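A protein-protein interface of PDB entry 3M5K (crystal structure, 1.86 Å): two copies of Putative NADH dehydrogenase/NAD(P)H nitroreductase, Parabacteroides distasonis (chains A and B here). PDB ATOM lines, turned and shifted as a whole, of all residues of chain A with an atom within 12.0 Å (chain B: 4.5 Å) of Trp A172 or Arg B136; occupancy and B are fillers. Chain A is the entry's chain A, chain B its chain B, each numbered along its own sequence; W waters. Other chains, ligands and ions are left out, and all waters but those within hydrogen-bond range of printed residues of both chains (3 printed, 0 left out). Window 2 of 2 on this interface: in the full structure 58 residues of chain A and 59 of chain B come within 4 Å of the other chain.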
ATOM      1  N   ASN A 163      -4.440  28.268  -9.648  1.00  0.00           N
ATOM      2  CA  ASN A 163      -4.815  27.356  -8.548  1.00  0.00           C
ATOM      3  C   ASN A 163      -3.963  26.084  -8.648  1.00  0.00           C
ATOM      4  O   ASN A 163      -4.189  25.256  -9.533  1.00  0.00           O
ATOM      5  CB  ASN A 163      -6.318  27.012  -8.624  1.00  0.00           C
ATOM      6  CG  ASN A 163      -6.764  26.034  -7.550  1.00  0.00           C
ATOM      7  OD1 ASN A 163      -5.979  25.665  -6.669  1.00  0.00           O
ATOM      8  ND2 ASN A 163      -8.038  25.614  -7.608  1.00  0.00           N
ATOM      9  N   VAL A 164      -2.915  25.999  -7.816  1.00  0.00           N
ATOM     10  CA  VAL A 164      -1.927  24.923  -7.920  1.00  0.00           C
ATOM     11  C   VAL A 164      -2.581  23.567  -7.733  1.00  0.00           C
ATOM     12  O   VAL A 164      -2.073  22.543  -8.204  1.00  0.00           O
ATOM     13  CB  VAL A 164      -0.780  25.082  -6.879  1.00  0.00           C
ATOM     14  CG1 VAL A 164      -1.290  24.734  -5.465  1.00  0.00           C
ATOM     15  CG2 VAL A 164       0.429  24.223  -7.286  1.00  0.00           C
ATOM     16  N   GLN A 165      -3.738  23.580  -7.085  1.00  0.00           N
ATOM     17  CA  GLN A 165      -4.512  22.361  -6.839  1.00  0.00           C
ATOM     18  C   GLN A 165      -5.215  21.793  -8.085  1.00  0.00           C
ATOM     19  O   GLN A 165      -5.797  20.704  -8.029  1.00  0.00           O
ATOM     20  CB  GLN A 165      -5.548  22.617  -5.748  1.00  0.00           C
ATOM     21  CG  GLN A 165      -4.950  23.053  -4.384  1.00  0.00           C
ATOM     22  CD  GLN A 165      -4.037  21.992  -3.773  1.00  0.00           C
ATOM     23  OE1 GLN A 165      -2.973  22.311  -3.233  1.00  0.00           O
ATOM     24  NE2 GLN A 165      -4.445  20.723  -3.865  1.00  0.00           N
ATOM     25  N   GLN A 166      -5.183  22.542  -9.185  1.00  0.00           N
ATOM     26  CA  GLN A 166      -5.634  22.019 -10.478  1.00  0.00           C
ATOM     27  C   GLN A 166      -4.448  21.602 -11.371  1.00  0.00           C
ATOM     28  O   GLN A 166      -4.585  21.461 -12.598  1.00  0.00           O
ATOM     29  CB  GLN A 166      -6.582  23.021 -11.149  1.00  0.00           C
ATOM     30  CG  GLN A 166      -7.923  23.116 -10.412  1.00  0.00           C
ATOM     31  CD  GLN A 166      -8.772  24.314 -10.814  1.00  0.00           C
ATOM     32  OE1 GLN A 166      -8.531  25.446 -10.385  1.00  0.00           O
ATOM     33  NE2 GLN A 166      -9.791  24.060 -11.612  1.00  0.00           N
ATOM     34  N   ILE A 167      -3.294  21.363 -10.729  1.00  0.00           N
ATOM     35  CA  ILE A 167      -2.116  20.783 -11.380  1.00  0.00           C
ATOM     36  C   ILE A 167      -1.826  19.380 -10.802  1.00  0.00           C
ATOM     37  O   ILE A 167      -1.851  19.189  -9.588  1.00  0.00           O
ATOM     38  CB  ILE A 167      -0.868  21.671 -11.192  1.00  0.00           C
ATOM     39  CG1 ILE A 167      -1.131  23.095 -11.722  1.00  0.00           C
ATOM     40  CG2 ILE A 167       0.354  21.011 -11.868  1.00  0.00           C
ATOM     41  CD1 ILE A 167       0.017  24.054 -11.581  1.00  0.00           C
ATOM     42  N   HIS A 168      -1.581  18.409 -11.684  1.00  0.00           N
ATOM     43  CA  HIS A 168      -1.347  17.025 -11.320  1.00  0.00           C
ATOM     44  C   HIS A 168      -0.127  16.554 -12.087  1.00  0.00           C
ATOM     45  O   HIS A 168       0.196  17.069 -13.158  1.00  0.00           O
ATOM     46  CB  HIS A 168      -2.562  16.134 -11.678  1.00  0.00           C
ATOM     47  CG  HIS A 168      -3.874  16.647 -11.180  1.00  0.00           C
ATOM     48  ND1 HIS A 168      -4.605  15.998 -10.201  1.00  0.00           N
ATOM     49  CD2 HIS A 168      -4.623  17.705 -11.565  1.00  0.00           C
ATOM     50  CE1 HIS A 168      -5.714  16.677  -9.966  1.00  0.00           C
ATOM     51  NE2 HIS A 168      -5.733  17.734 -10.763  1.00  0.00           N
ATOM     52  N   HIS A 169       0.571  15.577 -11.536  1.00  0.00           N
ATOM     53  CA  HIS A 169       1.788  15.041 -12.138  1.00  0.00           C
ATOM     54  C   HIS A 169       1.675  13.543 -12.353  1.00  0.00           C
ATOM     55  O   HIS A 169       1.463  12.787 -11.407  1.00  0.00           O
ATOM     56  CB  HIS A 169       2.997  15.364 -11.230  1.00  0.00           C
ATOM     57  CG  HIS A 169       3.304  16.826 -11.147  1.00  0.00           C
ATOM     58  ND1 HIS A 169       2.688  17.666 -10.245  1.00  0.00           N
ATOM     59  CD2 HIS A 169       4.134  17.600 -11.879  1.00  0.00           C
ATOM     60  CE1 HIS A 169       3.141  18.891 -10.414  1.00  0.00           C
ATOM     61  NE2 HIS A 169       4.021  18.877 -11.395  1.00  0.00           N
ATOM     62  N   ASN A 170       1.715  13.133 -13.618  1.00  0.00           N
ATOM     63  CA  ASN A 170       1.763  11.745 -14.057  1.00  0.00           C
ATOM     64  C   ASN A 170       0.511  10.907 -13.822  1.00  0.00           C
ATOM     65  O   ASN A 170       0.498   9.724 -14.104  1.00  0.00           O
ATOM     66  CB  ASN A 170       3.027  11.036 -13.526  1.00  0.00           C
ATOM     67  CG  ASN A 170       4.273  11.403 -14.337  1.00  0.00           C
ATOM     68  OD1 ASN A 170       4.196  11.671 -15.549  1.00  0.00           O
ATOM     69  ND2 ASN A 170       5.440  11.364 -13.683  1.00  0.00           N
ATOM     70  N   GLY A 171      -0.552  11.565 -13.402  1.00  0.00           N
ATOM     71  CA  GLY A 171      -1.798  10.920 -13.091  1.00  0.00           C
ATOM     72  C   GLY A 171      -2.554  11.864 -12.185  1.00  0.00           C
ATOM     73  O   GLY A 171      -2.010  12.888 -11.716  1.00  0.00           O
ATOM     74  N   TRP A 172      -3.828  11.551 -11.979  1.00  0.00           N
ATOM     75  CA  TRP A 172      -4.677  12.332 -11.103  1.00  0.00           C
ATOM     76  C   TRP A 172      -4.037  12.496  -9.712  1.00  0.00           C
ATOM     77  O   TRP A 172      -3.508  11.500  -9.158  1.00  0.00           O
ATOM     78  CB  TRP A 172      -6.059  11.694 -10.995  1.00  0.00           C
ATOM     79  CG  TRP A 172      -6.987  12.512 -10.189  1.00  0.00           C
ATOM     80  CD1 TRP A 172      -7.415  12.241  -8.936  1.00  0.00           C
ATOM     81  CD2 TRP A 172      -7.615  13.754 -10.581  1.00  0.00           C
ATOM     82  NE1 TRP A 172      -8.295  13.212  -8.522  1.00  0.00           N
ATOM     83  CE2 TRP A 172      -8.424  14.162  -9.507  1.00  0.00           C
ATOM     84  CE3 TRP A 172      -7.579  14.547 -11.739  1.00  0.00           C
ATOM     85  CZ2 TRP A 172      -9.182  15.329  -9.539  1.00  0.00           C
ATOM     86  CZ3 TRP A 172      -8.352  15.700 -11.787  1.00  0.00           C
ATOM     87  CH2 TRP A 172      -9.141  16.092 -10.684  1.00  0.00           C
ATOM     88  OXT TRP A 172      -4.008  13.600  -9.141  1.00  0.00           O
ATOM     89  N   GLU B  51      -8.599  20.908 -15.267  1.00  0.00           N
ATOM     90  CA  GLU B  51      -7.549  20.189 -14.530  1.00  0.00           C
ATOM     91  C   GLU B  51      -6.428  19.886 -15.525  1.00  0.00           C
ATOM     92  O   GLU B  51      -6.694  19.492 -16.667  1.00  0.00           O
ATOM     93  CB  GLU B  51      -8.111  18.881 -13.929  1.00  0.00           C
ATOM     94  CG  GLU B  51      -9.274  19.068 -12.962  1.00  0.00           C
ATOM     95  CD  GLU B  51      -8.878  19.561 -11.583  1.00  0.00           C
ATOM     96  OE1 GLU B  51      -7.678  19.520 -11.228  1.00  0.00           O
ATOM     97  OE2 GLU B  51      -9.789  20.008 -10.858  1.00  0.00           O
ATOM     98  N   ILE B  53      -2.797  17.753 -16.266  1.00  0.00           N
ATOM     99  CA  ILE B  53      -1.923  16.653 -15.878  1.00  0.00           C
ATOM    100  C   ILE B  53      -0.623  16.856 -16.652  1.00  0.00           C
ATOM    101  O   ILE B  53      -0.583  16.768 -17.890  1.00  0.00           O
ATOM    102  CB  ILE B  53      -2.493  15.191 -16.191  1.00  0.00           C
ATOM    103  CG1 ILE B  53      -4.008  15.071 -15.966  1.00  0.00           C
ATOM    104  CG2 ILE B  53      -1.708  14.071 -15.406  1.00  0.00           C
ATOM    105  CD1 ILE B  53      -4.505  15.347 -14.621  1.00  0.00           C
ATOM    106  N   ARG B 132      -7.875   7.892 -19.718  1.00  0.00           N
ATOM    107  CA  ARG B 132      -8.448   7.692 -18.409  1.00  0.00           C
ATOM    108  C   ARG B 132      -7.685   6.576 -17.642  1.00  0.00           C
ATOM    109  O   ARG B 132      -7.396   6.738 -16.474  1.00  0.00           O
ATOM    110  CB  ARG B 132      -9.935   7.316 -18.479  1.00  0.00           C
ATOM    111  CG  ARG B 132     -10.529   6.857 -17.136  1.00  0.00           C
ATOM    112  CD  ARG B 132     -12.054   6.693 -17.132  1.00  0.00           C
ATOM    113  NE  ARG B 132     -12.749   7.743 -17.891  1.00  0.00           N
ATOM    114  CZ  ARG B 132     -12.909   8.988 -17.455  1.00  0.00           C
ATOM    115  NH1 ARG B 132     -12.410   9.378 -16.290  1.00  0.00           N
ATOM    116  NH2 ARG B 132     -13.537   9.861 -18.219  1.00  0.00           N
ATOM    117  N   LYS B 133      -7.415   5.469 -18.303  1.00  0.00           N
ATOM    118  CA  LYS B 133      -6.823   4.327 -17.607  1.00  0.00           C
ATOM    119  C   LYS B 133      -5.336   4.575 -17.359  1.00  0.00           C
ATOM    120  O   LYS B 133      -4.808   4.234 -16.259  1.00  0.00           O
ATOM    121  CB  LYS B 133      -7.081   3.038 -18.378  1.00  0.00           C
ATOM    122  CG  LYS B 133      -8.538   2.590 -18.202  1.00  0.00           C
ATOM    123  CD  LYS B 133      -8.852   1.451 -19.123  1.00  0.00           C
ATOM    124  CE  LYS B 133     -10.270   0.898 -18.856  1.00  0.00           C
ATOM    125  NZ  LYS B 133     -10.511  -0.301 -19.729  1.00  0.00           N
ATOM    126  N   GLU B 134      -4.678   5.232 -18.307  1.00  0.00           N
ATOM    127  CA  GLU B 134      -3.247   5.547 -18.122  1.00  0.00           C
ATOM    128  C   GLU B 134      -2.995   6.512 -16.982  1.00  0.00           C
ATOM    129  O   GLU B 134      -2.031   6.323 -16.201  1.00  0.00           O
ATOM    130  CB  GLU B 134      -2.564   6.002 -19.418  1.00  0.00           C
ATOM    131  CG  GLU B 134      -1.033   6.168 -19.305  1.00  0.00           C
ATOM    132  CD  GLU B 134      -0.310   4.867 -18.921  1.00  0.00           C
ATOM    133  OE1 GLU B 134      -0.724   3.780 -19.404  1.00  0.00           O
ATOM    134  OE2 GLU B 134       0.678   4.962 -18.131  1.00  0.00           O
ATOM    135  N   LEU B 135      -3.871   7.509 -16.821  1.00  0.00           N
ATOM    136  CA  LEU B 135      -3.681   8.601 -15.882  1.00  0.00           C
ATOM    137  C   LEU B 135      -4.551   8.512 -14.640  1.00  0.00           C
ATOM    138  O   LEU B 135      -4.521   9.391 -13.814  1.00  0.00           O
ATOM    139  CB  LEU B 135      -3.832   9.996 -16.588  1.00  0.00           C
ATOM    140  CG  LEU B 135      -2.885  10.216 -17.794  1.00  0.00           C
ATOM    141  CD1 LEU B 135      -3.048  11.637 -18.418  1.00  0.00           C
ATOM    142  CD2 LEU B 135      -1.377   9.997 -17.427  1.00  0.00           C
ATOM    143  N   ARG B 136      -5.274   7.399 -14.492  1.00  0.00           N
ATOM    144  CA  ARG B 136      -6.109   7.119 -13.312  1.00  0.00           C
ATOM    145  C   ARG B 136      -7.096   8.234 -13.025  1.00  0.00           C
ATOM    146  O   ARG B 136      -7.279   8.685 -11.887  1.00  0.00           O
ATOM    147  CB  ARG B 136      -5.207   6.745 -12.112  1.00  0.00           C
ATOM    148  CG  ARG B 136      -4.496   5.417 -12.435  1.00  0.00           C
ATOM    149  CD  ARG B 136      -3.415   5.056 -11.431  1.00  0.00           C
ATOM    150  NE  ARG B 136      -2.194   5.800 -11.639  1.00  0.00           N
ATOM    151  CZ  ARG B 136      -1.059   5.632 -10.947  1.00  0.00           C
ATOM    152  NH1 ARG B 136      -0.987   4.759  -9.938  1.00  0.00           N
ATOM    153  NH2 ARG B 136      -0.004   6.354 -11.258  1.00  0.00           N
ATOM    154  N   LEU B 137      -7.755   8.685 -14.104  1.00  0.00           N
ATOM    155  CA  LEU B 137      -8.671   9.816 -13.992  1.00  0.00           C
ATOM    156  C   LEU B 137     -10.004   9.343 -13.430  1.00  0.00           C
ATOM    157  O   LEU B 137     -10.590   8.404 -13.955  1.00  0.00           O
ATOM    158  CB  LEU B 137      -8.914  10.465 -15.353  1.00  0.00           C
ATOM    159  CG  LEU B 137      -7.713  11.054 -16.086  1.00  0.00           C
ATOM    160  CD1 LEU B 137      -8.139  11.669 -17.464  1.00  0.00           C
ATOM    161  CD2 LEU B 137      -6.946  12.066 -15.204  1.00  0.00           C
ATOM    162  N   PRO B 138     -10.469   9.969 -12.360  1.00  0.00           N
ATOM    163  CA  PRO B 138     -11.792   9.672 -11.835  1.00  0.00           C
ATOM    164  C   PRO B 138     -12.865   9.869 -12.888  1.00  0.00           C
ATOM    165  O   PRO B 138     -12.694  10.687 -13.788  1.00  0.00           O
ATOM    166  CB  PRO B 138     -11.974  10.694 -10.717  1.00  0.00           C
ATOM    167  CG  PRO B 138     -10.626  11.098 -10.330  1.00  0.00           C
ATOM    168  CD  PRO B 138      -9.772  10.973 -11.562  1.00  0.00           C
ATOM    169  N   ILE B 141     -13.963  13.265 -14.271  1.00  0.00           N
ATOM    170  CA  ILE B 141     -12.929  14.032 -14.943  1.00  0.00           C
ATOM    171  C   ILE B 141     -12.838  13.493 -16.367  1.00  0.00           C
ATOM    172  O   ILE B 141     -12.634  12.295 -16.570  1.00  0.00           O
ATOM    173  CB  ILE B 141     -11.562  13.927 -14.192  1.00  0.00           C
ATOM    174  CG1 ILE B 141     -11.710  14.411 -12.753  1.00  0.00           C
ATOM    175  CG2 ILE B 141     -10.438  14.692 -14.944  1.00  0.00           C
ATOM    176  CD1 ILE B 141     -12.170  15.858 -12.599  1.00  0.00           C
HETATM  177  O   HOH W   1     -11.504  22.004 -11.739  1.00  0.00           O
HETATM  178  O   HOH W   2      -8.657  20.180  -8.456  1.00  0.00           O
HETATM  179  O   HOH W   3      -1.093   7.519 -13.779  1.00  0.00           O
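NE2 of His A168 is in hydrogen-bond range of OE1 of Glu B51 (2.7 Å). The backbone NH (N) of Trp A172 sits at hydrogen-bond distance from the backbone carbonyl oxygen (O) of Leu B135, at 2.9 Å.
N of Gln A165 lies close to OD1 of Asn A163 (3.1 Å). The side-chain amide nitrogen of Asn A163 is in hydrogen-bond range of the side-chain amide oxygen of Gln A166 (2.8 Å). ND1 of His A168 sits at hydrogen-bond distance from OXT of Trp A172 (2.7 Å). The guanidinium group (NH1) of Arg B132 lies within hydrogen-bond range of the backbone carbonyl oxygen (O) of Pro B138 (2.8 Å). The guanidinium group of Arg B132 sits at hydrogen-bond distance from the backbone carbonyl oxygen of Ile B141 (2.9 Å).
Glu B51 touches Gln A165. OE1 of Glu B51 touches CA of Gln A166, at 3.3 Å. His A168 touches Ile B53 (O to CA, 3.5 Å). Ile B53 touches Asn A170. Leu B135 touches Asn A170 (CD2 to O, 3.8 Å). Ile B53 touches Gly A171 (CG2 to N, 3.4 Å). CA of Gly A171 touches O of Leu B135 (3.2 Å). Trp A172 touches Glu B51 (CH2 to CD, 3.6 Å). CB of Trp A172 touches O of Arg B136, 3.4 Å away. Trp A172 touches Ile B141 (CH2 to CD1, 3.6 Å).
Of the printed residues of chain B, Gln A165 touches Glu B51 (3.9 Å). Of the printed residues of chain B, Gln A166 touches Glu B51. Printed residues of chain B within 4 Å of His A168: Glu B51 and Ile B53. Of chain A, only Asn A170 (3.8 Å), Gly A171 (3.2 Å) and Trp A172 (2.9 Å) come within 4 Å of Leu B135. Of chain A, only Trp A172 (3.4 Å) comes within 4 Å of Arg B136. No residue of chain A comes within 4 Å of Leu B137. Ile B141 touches just one residue of chain A: Trp A172 (3.6 Å). The nearest printed residue of chain B that does not touch Trp A172 is Ile B53 (4.3 Å).
Of the 10 printed residues of chain A, 6 touch a printed residue of chain B. Hydrophobic or aromatic side chains of chain A within 4 Å of the printed part of chain B: His A168 and Trp A172. Printed residues of chain B that touch a printed residue of chain A: Glu B51, Ile B53, Leu B135, Arg B136, Pro B138 and Ile B141. Hydrophobic or aromatic side chains of chain B within 4 Å of the printed part of chain A: Ile B53, Leu B135, Pro B138 and Ile B141. Among the printed residues, no Asp or Glu carboxylate lies within 4 Å of a Lys or Arg side-chain nitrogen of the other chain.
No position is printed for both chains.
Water W2 bridges OE2 of Glu B51 and O of Gln A165. Water W1 bridges the side-chain amide nitrogen of Gln A166 (2.7 Å) and the side-chain carboxylate of Glu B51 (2.8 Å). Water W3 lies within hydrogen-bond range of the backbone carbonyl oxygen of Asn A170 (2.7 Å), the backbone carbonyl oxygen of Glu B134 (2.9 Å) and the guanidinium group of Arg B136 (3.0 Å).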
